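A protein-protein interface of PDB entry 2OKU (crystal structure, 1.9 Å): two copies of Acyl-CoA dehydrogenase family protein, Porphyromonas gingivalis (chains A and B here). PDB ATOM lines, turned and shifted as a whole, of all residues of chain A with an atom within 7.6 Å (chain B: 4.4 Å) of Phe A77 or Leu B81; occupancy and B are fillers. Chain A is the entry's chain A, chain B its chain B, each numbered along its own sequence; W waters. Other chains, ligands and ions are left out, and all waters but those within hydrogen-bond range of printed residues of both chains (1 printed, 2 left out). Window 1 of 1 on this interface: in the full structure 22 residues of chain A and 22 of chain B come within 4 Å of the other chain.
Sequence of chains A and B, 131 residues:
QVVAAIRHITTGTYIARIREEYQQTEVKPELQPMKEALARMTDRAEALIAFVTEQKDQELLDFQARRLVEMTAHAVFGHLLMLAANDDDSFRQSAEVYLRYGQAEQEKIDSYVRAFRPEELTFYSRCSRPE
Printed residues of chain B within 4 Å of Tyr A14: Phe B91 (3.3 Å). Of the printed residues of chain B, Glu A70 touches Ser B94 (3.7 Å). Of chain B, only Leu B81 (3.5 Å), Ala B84 (3.9 Å), Phe B91 (3.9 Å), Ser B94 (3.8 Å), Ala B95 (3.7 Å) and Tyr B98 (3.5 Å) come within 4 Å of Phe A77. Printed residues of chain B within 4 Å of Tyr A101: Tyr B98 (3.7 Å). Leu B81 touches one residue of chain A. Printed residues of chain A within 4 Å of Phe B91: Tyr A14 (3.3 Å), Ala A73 (3.8 Å) and Phe A77 (3.9 Å). Of the printed residues of chain A, Ser B94 touches Glu A70 (3.7 Å), Ala A73 (3.5 Å) and Phe A77 (3.8 Å). The nearest residue of chain A that does not touch Leu B81 is Leu A80 (4.2 Å).
CE2 of Phe B91 touches CZ of Tyr A14 (3.3 Å). Ser B94 touches Glu A70. CE1 of Phe B91 touches CB of Ala A73, at 3.8 Å. Phe A77 touches Ala B84. Phe B91 touches Phe A77 (CD2 to CE1, 3.9 Å). N of Ala B95 touches CE2 of Phe A77, 3.7 Å away. Phe A77 touches Tyr B98 (CD2 to CE1, 3.5 Å). Leu A80 touches Ala B84 (CD1 to CB, 3.8 Å). CD2 of Leu A81 touches CG of Phe B77 (3.6 Å). Tyr B98 touches Gly A102 (OH to CA, 3.7 Å).
Along chain A the printed residues that touch a printed residue of chain B span positions 14 to 102. Among the printed residues, 17 pairs touch across the chains.
Water W1 lies within hydrogen-bond range of the backbone carbonyl oxygen (O) of Ala B84 (2.8 Å) and the side-chain hydroxyl (OH) of Tyr A14 (2.9 Å).
Phe A77 touches Leu B81, and with the chains exchanged Leu A81 touches Phe B77. Phe A77 touches Tyr B98, and with the chains exchanged Tyr A98 touches Phe B77. Tyr A98 touches its own counterpart, Tyr B98. 8 positions are printed for both chains.
A ring nitrogen (ND1) of His A74 sits at hydrogen-bond distance from the side-chain hydroxyl (OH) of Tyr B98 (2.7 Å).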
ATOM      1  N   TYR A  14     -18.290  28.612 -33.084  1.00  0.00           N
ATOM      2  CA  TYR A  14     -18.864  28.533 -31.737  1.00  0.00           C
ATOM      3  C   TYR A  14     -20.245  29.162 -31.649  1.00  0.00           C
ATOM      4  O   TYR A  14     -21.091  28.709 -30.876  1.00  0.00           O
ATOM      5  CB  TYR A  14     -17.989  29.222 -30.706  1.00  0.00           C
ATOM      6  CG  TYR A  14     -16.733  28.505 -30.334  1.00  0.00           C
ATOM      7  CD1 TYR A  14     -16.769  27.391 -29.495  1.00  0.00           C
ATOM      8  CD2 TYR A  14     -15.494  28.943 -30.787  1.00  0.00           C
ATOM      9  CE1 TYR A  14     -15.596  26.742 -29.114  1.00  0.00           C
ATOM     10  CE2 TYR A  14     -14.324  28.304 -30.418  1.00  0.00           C
ATOM     11  CZ  TYR A  14     -14.377  27.214 -29.581  1.00  0.00           C
ATOM     12  OH  TYR A  14     -13.202  26.586 -29.216  1.00  0.00           O
ATOM     13  N   ILE A  18     -23.431  27.214 -30.247  1.00  0.00           N
ATOM     14  CA  ILE A  18     -24.282  27.846 -29.269  1.00  0.00           C
ATOM     15  C   ILE A  18     -25.741  27.804 -29.736  1.00  0.00           C
ATOM     16  O   ILE A  18     -26.628  27.386 -28.990  1.00  0.00           O
ATOM     17  CB  ILE A  18     -23.867  29.317 -29.025  1.00  0.00           C
ATOM     18  CG1 ILE A  18     -22.612  29.332 -28.114  1.00  0.00           C
ATOM     19  CG2 ILE A  18     -25.073  30.112 -28.428  1.00  0.00           C
ATOM     20  CD1 ILE A  18     -21.935  30.690 -27.993  1.00  0.00           C
ATOM     21  N   TYR A  22     -26.332  24.372 -27.749  1.00  0.00           N
ATOM     22  CA  TYR A  22     -26.468  24.814 -26.350  1.00  0.00           C
ATOM     23  C   TYR A  22     -27.781  25.557 -26.094  1.00  0.00           C
ATOM     24  O   TYR A  22     -28.418  25.373 -25.049  1.00  0.00           O
ATOM     25  CB  TYR A  22     -25.301  25.680 -25.925  1.00  0.00           C
ATOM     26  CG  TYR A  22     -23.938  25.057 -26.010  1.00  0.00           C
ATOM     27  CD1 TYR A  22     -23.742  23.688 -25.860  1.00  0.00           C
ATOM     28  CD2 TYR A  22     -22.812  25.856 -26.230  1.00  0.00           C
ATOM     29  CE1 TYR A  22     -22.471  23.130 -25.947  1.00  0.00           C
ATOM     30  CE2 TYR A  22     -21.540  25.303 -26.291  1.00  0.00           C
ATOM     31  CZ  TYR A  22     -21.370  23.945 -26.143  1.00  0.00           C
ATOM     32  OH  TYR A  22     -20.097  23.407 -26.209  1.00  0.00           O
ATOM     33  N   MET A  34     -30.968  33.300 -17.673  1.00  0.00           N
ATOM     34  CA  MET A  34     -29.579  33.147 -18.025  1.00  0.00           C
ATOM     35  C   MET A  34     -29.429  32.689 -19.471  1.00  0.00           C
ATOM     36  O   MET A  34     -28.577  33.201 -20.181  1.00  0.00           O
ATOM     37  CB  MET A  34     -28.827  32.185 -17.102  1.00  0.00           C
ATOM     38  CG  MET A  34     -27.361  32.073 -17.487  1.00  0.00           C
ATOM     39  SD  MET A  34     -26.358  31.069 -16.093  1.00  0.00           S
ATOM     40  CE  MET A  34     -24.532  31.424 -16.807  1.00  0.00           C
ATOM     41  N   LEU A  38     -27.416  34.818 -22.324  1.00  0.00           N
ATOM     42  CA  LEU A  38     -26.344  34.213 -23.104  1.00  0.00           C
ATOM     43  C   LEU A  38     -26.593  34.320 -24.598  1.00  0.00           C
ATOM     44  O   LEU A  38     -25.656  34.481 -25.354  1.00  0.00           O
ATOM     45  CB  LEU A  38     -26.151  32.752 -22.720  1.00  0.00           C
ATOM     46  CG  LEU A  38     -25.526  32.573 -21.338  1.00  0.00           C
ATOM     47  CD1 LEU A  38     -25.716  31.131 -20.882  1.00  0.00           C
ATOM     48  CD2 LEU A  38     -24.071  32.969 -21.350  1.00  0.00           C
ATOM     49  N   MET A  41     -25.534  37.780 -25.472  1.00  0.00           N
ATOM     50  CA  MET A  41     -24.043  37.827 -25.524  1.00  0.00           C
ATOM     51  C   MET A  41     -23.489  37.197 -26.815  1.00  0.00           C
ATOM     52  O   MET A  41     -22.481  37.664 -27.369  1.00  0.00           O
ATOM     53  CB  MET A  41     -23.420  37.123 -24.315  1.00  0.00           C
ATOM     54  CG  MET A  41     -23.690  37.823 -23.012  1.00  0.00           C
ATOM     55  SD  MET A  41     -23.051  36.786 -21.504  1.00  0.00           S
ATOM     56  CE  MET A  41     -21.138  37.014 -21.839  1.00  0.00           C
ATOM     57  N   GLU A  70     -11.693  36.696 -27.250  1.00  0.00           N
ATOM     58  CA  GLU A  70     -12.218  36.915 -25.912  1.00  0.00           C
ATOM     59  C   GLU A  70     -13.728  37.156 -25.887  1.00  0.00           C
ATOM     60  O   GLU A  70     -14.431  36.604 -25.045  1.00  0.00           O
ATOM     61  CB  GLU A  70     -11.527  38.093 -25.260  1.00  0.00           C
ATOM     62  CG  GLU A  70     -10.089  37.843 -24.931  1.00  0.00           C
ATOM     63  CD  GLU A  70      -9.466  39.104 -24.333  1.00  0.00           C
ATOM     64  OE1 GLU A  70     -10.100  39.692 -23.387  1.00  0.00           O
ATOM     65  OE2 GLU A  70      -8.382  39.486 -24.817  1.00  0.00           O
ATOM     66  N   MET A  71     -14.200  37.983 -26.820  1.00  0.00           N
ATOM     67  CA  MET A  71     -15.609  38.309 -26.938  1.00  0.00           C
ATOM     68  C   MET A  71     -16.416  37.014 -27.110  1.00  0.00           C
ATOM     69  O   MET A  71     -17.465  36.802 -26.477  1.00  0.00           O
ATOM     70  CB  MET A  71     -15.807  39.248 -28.136  1.00  0.00           C
ATOM     71  CG  MET A  71     -17.192  39.811 -28.252  1.00  0.00           C
ATOM     72  SD  MET A  71     -17.404  41.277 -26.913  1.00  0.00           S
ATOM     73  CE  MET A  71     -19.301  41.693 -27.364  1.00  0.00           C
ATOM     74  N   THR A  72     -15.898  36.122 -27.947  1.00  0.00           N
ATOM     75  CA  THR A  72     -16.512  34.833 -28.159  1.00  0.00           C
ATOM     76  C   THR A  72     -16.437  33.924 -26.931  1.00  0.00           C
ATOM     77  O   THR A  72     -17.432  33.257 -26.596  1.00  0.00           O
ATOM     78  CB  THR A  72     -15.886  34.129 -29.411  1.00  0.00           C
ATOM     79  OG1 THR A  72     -16.029  34.988 -30.565  1.00  0.00           O
ATOM     80  CG2 THR A  72     -16.586  32.796 -29.665  1.00  0.00           C
ATOM     81  N   ALA A  73     -15.260  33.858 -26.311  1.00  0.00           N
ATOM     82  CA  ALA A  73     -15.010  33.057 -25.117  1.00  0.00           C
ATOM     83  C   ALA A  73     -16.033  33.365 -24.013  1.00  0.00           C
ATOM     84  O   ALA A  73     -16.570  32.452 -23.359  1.00  0.00           O
ATOM     85  CB  ALA A  73     -13.561  33.284 -24.600  1.00  0.00           C
ATOM     86  N   HIS A  74     -16.339  34.643 -23.797  1.00  0.00           N
ATOM     87  CA  HIS A  74     -17.313  34.997 -22.752  1.00  0.00           C
ATOM     88  C   HIS A  74     -18.671  34.330 -22.996  1.00  0.00           C
ATOM     89  O   HIS A  74     -19.291  33.779 -22.060  1.00  0.00           O
ATOM     90  CB  HIS A  74     -17.443  36.521 -22.586  1.00  0.00           C
ATOM     91  CG  HIS A  74     -16.198  37.153 -22.074  1.00  0.00           C
ATOM     92  ND1 HIS A  74     -15.636  36.792 -20.871  1.00  0.00           N
ATOM     93  CD2 HIS A  74     -15.380  38.081 -22.615  1.00  0.00           C
ATOM     94  CE1 HIS A  74     -14.503  37.456 -20.708  1.00  0.00           C
ATOM     95  NE2 HIS A  74     -14.344  38.273 -21.736  1.00  0.00           N
ATOM     96  N   ALA A  75     -19.135  34.358 -24.247  1.00  0.00           N
ATOM     97  CA  ALA A  75     -20.381  33.686 -24.606  1.00  0.00           C
ATOM     98  C   ALA A  75     -20.321  32.167 -24.475  1.00  0.00           C
ATOM     99  O   ALA A  75     -21.258  31.574 -23.947  1.00  0.00           O
ATOM    100  CB  ALA A  75     -20.820  34.081 -26.041  1.00  0.00           C
ATOM    101  N   VAL A  76     -19.251  31.539 -24.971  1.00  0.00           N
ATOM    102  CA  VAL A  76     -19.077  30.086 -24.872  1.00  0.00           C
ATOM    103  C   VAL A  76     -18.993  29.642 -23.430  1.00  0.00           C
ATOM    104  O   VAL A  76     -19.767  28.763 -22.986  1.00  0.00           O
ATOM    105  CB  VAL A  76     -17.832  29.607 -25.640  1.00  0.00           C
ATOM    106  CG1 VAL A  76     -17.559  28.080 -25.388  1.00  0.00           C
ATOM    107  CG2 VAL A  76     -17.973  29.933 -27.164  1.00  0.00           C
ATOM    108  N   PHE A  77     -18.088  30.278 -22.687  1.00  0.00           N
ATOM    109  CA  PHE A  77     -17.850  29.935 -21.277  1.00  0.00           C
ATOM    110  C   PHE A  77     -19.159  30.013 -20.510  1.00  0.00           C
ATOM    111  O   PHE A  77     -19.470  29.127 -19.711  1.00  0.00           O
ATOM    112  CB  PHE A  77     -16.824  30.882 -20.667  1.00  0.00           C
ATOM    113  CG  PHE A  77     -15.376  30.600 -21.056  1.00  0.00           C
ATOM    114  CD1 PHE A  77     -15.016  29.677 -22.038  1.00  0.00           C
ATOM    115  CD2 PHE A  77     -14.361  31.322 -20.430  1.00  0.00           C
ATOM    116  CE1 PHE A  77     -13.678  29.451 -22.351  1.00  0.00           C
ATOM    117  CE2 PHE A  77     -13.026  31.116 -20.753  1.00  0.00           C
ATOM    118  CZ  PHE A  77     -12.677  30.186 -21.716  1.00  0.00           C
ATOM    119  N   GLY A  78     -19.932  31.071 -20.762  1.00  0.00           N
ATOM    120  CA  GLY A  78     -21.196  31.301 -20.054  1.00  0.00           C
ATOM    121  C   GLY A  78     -22.160  30.152 -20.262  1.00  0.00           C
ATOM    122  O   GLY A  78     -22.855  29.686 -19.328  1.00  0.00           O
ATOM    123  N   HIS A  79     -22.197  29.655 -21.501  1.00  0.00           N
ATOM    124  CA  HIS A  79     -23.011  28.470 -21.798  1.00  0.00           C
ATOM    125  C   HIS A  79     -22.523  27.235 -21.055  1.00  0.00           C
ATOM    126  O   HIS A  79     -23.352  26.480 -20.573  1.00  0.00           O
ATOM    127  CB  HIS A  79     -23.070  28.197 -23.298  1.00  0.00           C
ATOM    128  CG  HIS A  79     -24.037  29.073 -24.036  1.00  0.00           C
ATOM    129  ND1 HIS A  79     -23.670  30.283 -24.573  1.00  0.00           N
ATOM    130  CD2 HIS A  79     -25.355  28.922 -24.308  1.00  0.00           C
ATOM    131  CE1 HIS A  79     -24.724  30.843 -25.149  1.00  0.00           C
ATOM    132  NE2 HIS A  79     -25.762  30.031 -25.010  1.00  0.00           N
ATOM    133  N   LEU A  80     -21.203  27.016 -20.959  1.00  0.00           N
ATOM    134  CA  LEU A  80     -20.698  25.843 -20.244  1.00  0.00           C
ATOM    135  C   LEU A  80     -21.129  25.874 -18.788  1.00  0.00           C
ATOM    136  O   LEU A  80     -21.516  24.849 -18.205  1.00  0.00           O
ATOM    137  CB  LEU A  80     -19.181  25.744 -20.340  1.00  0.00           C
ATOM    138  CG  LEU A  80     -18.616  25.673 -21.743  1.00  0.00           C
ATOM    139  CD1 LEU A  80     -17.077  25.691 -21.698  1.00  0.00           C
ATOM    140  CD2 LEU A  80     -19.129  24.424 -22.464  1.00  0.00           C
ATOM    141  N   LEU A  81     -21.106  27.068 -18.210  1.00  0.00           N
ATOM    142  CA  LEU A  81     -21.517  27.243 -16.818  1.00  0.00           C
ATOM    143  C   LEU A  81     -23.046  27.122 -16.647  1.00  0.00           C
ATOM    144  O   LEU A  81     -23.520  26.532 -15.679  1.00  0.00           O
ATOM    145  CB  LEU A  81     -20.973  28.575 -16.277  1.00  0.00           C
ATOM    146  CG  LEU A  81     -19.467  28.771 -16.391  1.00  0.00           C
ATOM    147  CD1 LEU A  81     -19.072  30.084 -15.591  1.00  0.00           C
ATOM    148  CD2 LEU A  81     -18.655  27.538 -15.961  1.00  0.00           C
ATOM    149  N   MET A  82     -23.808  27.632 -17.606  1.00  0.00           N
ATOM    150  CA  MET A  82     -25.264  27.410 -17.628  1.00  0.00           C
ATOM    151  C   MET A  82     -25.581  25.906 -17.630  1.00  0.00           C
ATOM    152  O   MET A  82     -26.473  25.451 -16.933  1.00  0.00           O
ATOM    153  CB  MET A  82     -25.900  28.085 -18.851  1.00  0.00           C
ATOM    154  CG  MET A  82     -27.373  28.456 -18.772  1.00  0.00           C
ATOM    155  SD  MET A  82     -28.289  28.079 -20.483  1.00  0.00           S
ATOM    156  CE  MET A  82     -27.973  26.342 -19.794  1.00  0.00           C
ATOM    157  N   LEU A  83     -24.862  25.146 -18.449  1.00  0.00           N
ATOM    158  CA  LEU A  83     -25.081  23.695 -18.525  1.00  0.00           C
ATOM    159  C   LEU A  83     -24.747  23.026 -17.197  1.00  0.00           C
ATOM    160  O   LEU A  83     -25.461  22.133 -16.769  1.00  0.00           O
ATOM    161  CB  LEU A  83     -24.295  23.103 -19.696  1.00  0.00           C
ATOM    162  CG  LEU A  83     -24.744  23.529 -21.109  1.00  0.00           C
ATOM    163  CD1 LEU A  83     -23.770  22.984 -22.153  1.00  0.00           C
ATOM    164  CD2 LEU A  83     -26.162  23.081 -21.457  1.00  0.00           C
ATOM    165  N   TYR A  98     -20.868  34.694 -12.516  1.00  0.00           N
ATOM    166  CA  TYR A  98     -19.960  34.572 -13.650  1.00  0.00           C
ATOM    167  C   TYR A  98     -20.572  35.208 -14.912  1.00  0.00           C
ATOM    168  O   TYR A  98     -19.858  35.812 -15.678  1.00  0.00           O
ATOM    169  CB  TYR A  98     -19.554  33.119 -13.938  1.00  0.00           C
ATOM    170  CG  TYR A  98     -18.352  32.611 -13.123  1.00  0.00           C
ATOM    171  CD1 TYR A  98     -18.451  32.386 -11.738  1.00  0.00           C
ATOM    172  CD2 TYR A  98     -17.123  32.399 -13.730  1.00  0.00           C
ATOM    173  CE1 TYR A  98     -17.369  31.936 -11.012  1.00  0.00           C
ATOM    174  CE2 TYR A  98     -16.041  31.956 -13.011  1.00  0.00           C
ATOM    175  CZ  TYR A  98     -16.166  31.710 -11.658  1.00  0.00           C
ATOM    176  OH  TYR A  98     -15.055  31.290 -10.965  1.00  0.00           O
ATOM    177  N   TYR A 101     -19.834  38.891 -14.841  1.00  0.00           N
ATOM    178  CA  TYR A 101     -18.437  39.060 -15.215  1.00  0.00           C
ATOM    179  C   TYR A 101     -18.279  39.033 -16.731  1.00  0.00           C
ATOM    180  O   TYR A 101     -17.688  39.936 -17.305  1.00  0.00           O
ATOM    181  CB  TYR A 101     -17.601  37.972 -14.583  1.00  0.00           C
ATOM    182  CG  TYR A 101     -16.133  38.019 -14.934  1.00  0.00           C
ATOM    183  CD1 TYR A 101     -15.274  38.908 -14.315  1.00  0.00           C
ATOM    184  CD2 TYR A 101     -15.617  37.189 -15.905  1.00  0.00           C
ATOM    185  CE1 TYR A 101     -13.904  38.949 -14.657  1.00  0.00           C
ATOM    186  CE2 TYR A 101     -14.288  37.231 -16.261  1.00  0.00           C
ATOM    187  CZ  TYR A 101     -13.428  38.095 -15.631  1.00  0.00           C
ATOM    188  OH  TYR A 101     -12.085  38.088 -16.009  1.00  0.00           O
ATOM    189  N   GLY A 102     -18.847  38.009 -17.368  1.00  0.00           N
ATOM    190  CA  GLY A 102     -18.787  37.886 -18.808  1.00  0.00           C
ATOM    191  C   GLY A 102     -19.447  39.064 -19.492  1.00  0.00           C
ATOM    192  O   GLY A 102     -18.936  39.588 -20.466  1.00  0.00           O
ATOM    193  N   PHE B  77     -16.198  25.137 -11.958  1.00  0.00           N
ATOM    194  CA  PHE B  77     -16.261  25.991 -13.153  1.00  0.00           C
ATOM    195  C   PHE B  77     -14.887  26.104 -13.814  1.00  0.00           C
ATOM    196  O   PHE B  77     -14.747  26.027 -15.051  1.00  0.00           O
ATOM    197  CB  PHE B  77     -16.729  27.388 -12.784  1.00  0.00           C
ATOM    198  CG  PHE B  77     -18.212  27.501 -12.432  1.00  0.00           C
ATOM    199  CD1 PHE B  77     -19.065  26.409 -12.391  1.00  0.00           C
ATOM    200  CD2 PHE B  77     -18.727  28.757 -12.128  1.00  0.00           C
ATOM    201  CE1 PHE B  77     -20.435  26.588 -12.060  1.00  0.00           C
ATOM    202  CE2 PHE B  77     -20.051  28.922 -11.776  1.00  0.00           C
ATOM    203  CZ  PHE B  77     -20.902  27.849 -11.758  1.00  0.00           C
ATOM    204  N   GLY B  78     -13.869  26.303 -12.985  1.00  0.00           N
ATOM    205  CA  GLY B  78     -12.496  26.381 -13.481  1.00  0.00           C
ATOM    206  C   GLY B  78     -12.085  25.189 -14.336  1.00  0.00           C
ATOM    207  O   GLY B  78     -11.459  25.348 -15.408  1.00  0.00           O
ATOM    208  N   HIS B  79     -12.439  23.990 -13.879  1.00  0.00           N
ATOM    209  CA  HIS B  79     -12.149  22.777 -14.653  1.00  0.00           C
ATOM    210  C   HIS B  79     -12.852  22.760 -16.006  1.00  0.00           C
ATOM    211  O   HIS B  79     -12.267  22.338 -16.984  1.00  0.00           O
ATOM    212  CB  HIS B  79     -12.504  21.525 -13.863  1.00  0.00           C
ATOM    213  CG  HIS B  79     -11.511  21.200 -12.788  1.00  0.00           C
ATOM    214  ND1 HIS B  79     -11.589  21.730 -11.517  1.00  0.00           N
ATOM    215  CD2 HIS B  79     -10.410  20.406 -12.802  1.00  0.00           C
ATOM    216  CE1 HIS B  79     -10.584  21.271 -10.792  1.00  0.00           C
ATOM    217  NE2 HIS B  79      -9.849  20.471 -11.548  1.00  0.00           N
ATOM    218  N   LEU B  80     -14.109  23.195 -16.042  1.00  0.00           N
ATOM    219  CA  LEU B  80     -14.879  23.219 -17.278  1.00  0.00           C
ATOM    220  C   LEU B  80     -14.213  24.147 -18.301  1.00  0.00           C
ATOM    221  O   LEU B  80     -14.148  23.844 -19.505  1.00  0.00           O
ATOM    222  CB  LEU B  80     -16.312  23.672 -16.993  1.00  0.00           C
ATOM    223  CG  LEU B  80     -17.167  22.809 -16.072  1.00  0.00           C
ATOM    224  CD1 LEU B  80     -18.576  23.467 -15.849  1.00  0.00           C
ATOM    225  CD2 LEU B  80     -17.269  21.423 -16.643  1.00  0.00           C
ATOM    226  N   LEU B  81     -13.699  25.266 -17.812  1.00  0.00           N
ATOM    227  CA  LEU B  81     -13.034  26.229 -18.690  1.00  0.00           C
ATOM    228  C   LEU B  81     -11.661  25.733 -19.130  1.00  0.00           C
ATOM    229  O   LEU B  81     -11.260  25.986 -20.269  1.00  0.00           O
ATOM    230  CB  LEU B  81     -12.958  27.585 -18.014  1.00  0.00           C
ATOM    231  CG  LEU B  81     -14.319  28.151 -17.583  1.00  0.00           C
ATOM    232  CD1 LEU B  81     -14.132  29.626 -17.121  1.00  0.00           C
ATOM    233  CD2 LEU B  81     -15.441  28.026 -18.671  1.00  0.00           C
ATOM    234  N   MET B  82     -10.947  25.014 -18.248  1.00  0.00           N
ATOM    235  CA  MET B  82      -9.715  24.357 -18.646  1.00  0.00           C
ATOM    236  C   MET B  82      -9.952  23.392 -19.793  1.00  0.00           C
ATOM    237  O   MET B  82      -9.171  23.358 -20.751  1.00  0.00           O
ATOM    238  CB  MET B  82      -9.049  23.555 -17.504  1.00  0.00           C
ATOM    239  CG  MET B  82      -7.856  22.668 -18.057  1.00  0.00           C
ATOM    240  SD  MET B  82      -7.033  21.718 -16.585  1.00  0.00           S
ATOM    241  CE  MET B  82      -8.457  20.477 -16.305  1.00  0.00           C
ATOM    242  N   LEU B  83     -10.999  22.583 -19.677  1.00  0.00           N
ATOM    243  CA  LEU B  83     -11.351  21.644 -20.745  1.00  0.00           C
ATOM    244  C   LEU B  83     -11.677  22.345 -22.071  1.00  0.00           C
ATOM    245  O   LEU B  83     -11.282  21.864 -23.141  1.00  0.00           O
ATOM    246  CB  LEU B  83     -12.488  20.721 -20.298  1.00  0.00           C
ATOM    247  CG  LEU B  83     -12.119  19.778 -19.139  1.00  0.00           C
ATOM    248  CD1 LEU B  83     -13.350  18.993 -18.727  1.00  0.00           C
ATOM    249  CD2 LEU B  83     -10.966  18.859 -19.522  1.00  0.00           C
ATOM    250  N   ALA B  84     -12.359  23.485 -22.002  1.00  0.00           N
ATOM    251  CA  ALA B  84     -12.610  24.316 -23.190  1.00  0.00           C
ATOM    252  C   ALA B  84     -11.299  24.754 -23.847  1.00  0.00           C
ATOM    253  O   ALA B  84     -11.147  24.700 -25.072  1.00  0.00           O
ATOM    254  CB  ALA B  84     -13.493  25.540 -22.839  1.00  0.00           C
ATOM    255  N   ALA B  85     -10.353  25.176 -23.025  1.00  0.00           N
ATOM    256  CA  ALA B  85      -9.040  25.611 -23.493  1.00  0.00           C
ATOM    257  C   ALA B  85      -8.202  24.446 -24.002  1.00  0.00           C
ATOM    258  O   ALA B  85      -7.443  24.585 -24.991  1.00  0.00           O
ATOM    259  CB  ALA B  85      -8.318  26.379 -22.353  1.00  0.00           C
ATOM    260  N   PHE B  91      -8.632  29.702 -26.538  1.00  0.00           N
ATOM    261  CA  PHE B  91      -9.252  30.023 -25.274  1.00  0.00           C
ATOM    262  C   PHE B  91      -8.376  29.929 -24.015  1.00  0.00           C
ATOM    263  O   PHE B  91      -8.871  30.177 -22.917  1.00  0.00           O
ATOM    264  CB  PHE B  91     -10.491  29.128 -25.092  1.00  0.00           C
ATOM    265  CG  PHE B  91     -11.669  29.498 -25.969  1.00  0.00           C
ATOM    266  CD1 PHE B  91     -11.706  30.683 -26.717  1.00  0.00           C
ATOM    267  CD2 PHE B  91     -12.774  28.654 -26.012  1.00  0.00           C
ATOM    268  CE1 PHE B  91     -12.846  30.989 -27.491  1.00  0.00           C
ATOM    269  CE2 PHE B  91     -13.892  28.960 -26.787  1.00  0.00           C
ATOM    270  CZ  PHE B  91     -13.917  30.118 -27.524  1.00  0.00           C
ATOM    271  N   SER B  94      -8.079  33.389 -22.081  1.00  0.00           N
ATOM    272  CA  SER B  94      -9.379  33.650 -21.454  1.00  0.00           C
ATOM    273  C   SER B  94      -9.616  32.727 -20.254  1.00  0.00           C
ATOM    274  O   SER B  94     -10.088  33.172 -19.215  1.00  0.00           O
ATOM    275  CB  SER B  94     -10.534  33.496 -22.443  1.00  0.00           C
ATOM    276  OG  SER B  94     -10.480  34.475 -23.464  1.00  0.00           O
ATOM    277  N   ALA B  95      -9.312  31.445 -20.400  1.00  0.00           N
ATOM    278  CA  ALA B  95      -9.476  30.515 -19.289  1.00  0.00           C
ATOM    279  C   ALA B  95      -8.594  30.935 -18.103  1.00  0.00           C
ATOM    280  O   ALA B  95      -9.030  30.862 -16.962  1.00  0.00           O
ATOM    281  CB  ALA B  95      -9.170  29.086 -19.701  1.00  0.00           C
ATOM    282  N   TYR B  98     -10.135  33.871 -16.239  1.00  0.00           N
ATOM    283  CA  TYR B  98     -11.258  33.401 -15.437  1.00  0.00           C
ATOM    284  C   TYR B  98     -10.772  32.673 -14.171  1.00  0.00           C
ATOM    285  O   TYR B  98     -11.347  32.846 -13.121  1.00  0.00           O
ATOM    286  CB  TYR B  98     -12.172  32.469 -16.243  1.00  0.00           C
ATOM    287  CG  TYR B  98     -13.285  33.166 -16.983  1.00  0.00           C
ATOM    288  CD1 TYR B  98     -13.051  33.843 -18.155  1.00  0.00           C
ATOM    289  CD2 TYR B  98     -14.591  33.119 -16.493  1.00  0.00           C
ATOM    290  CE1 TYR B  98     -14.089  34.483 -18.839  1.00  0.00           C
ATOM    291  CE2 TYR B  98     -15.627  33.728 -17.161  1.00  0.00           C
ATOM    292  CZ  TYR B  98     -15.379  34.417 -18.330  1.00  0.00           C
ATOM    293  OH  TYR B  98     -16.443  35.017 -18.961  1.00  0.00           O
HETATM  294  O   HOH W   1     -13.383  25.113 -26.781  1.00  0.00           O
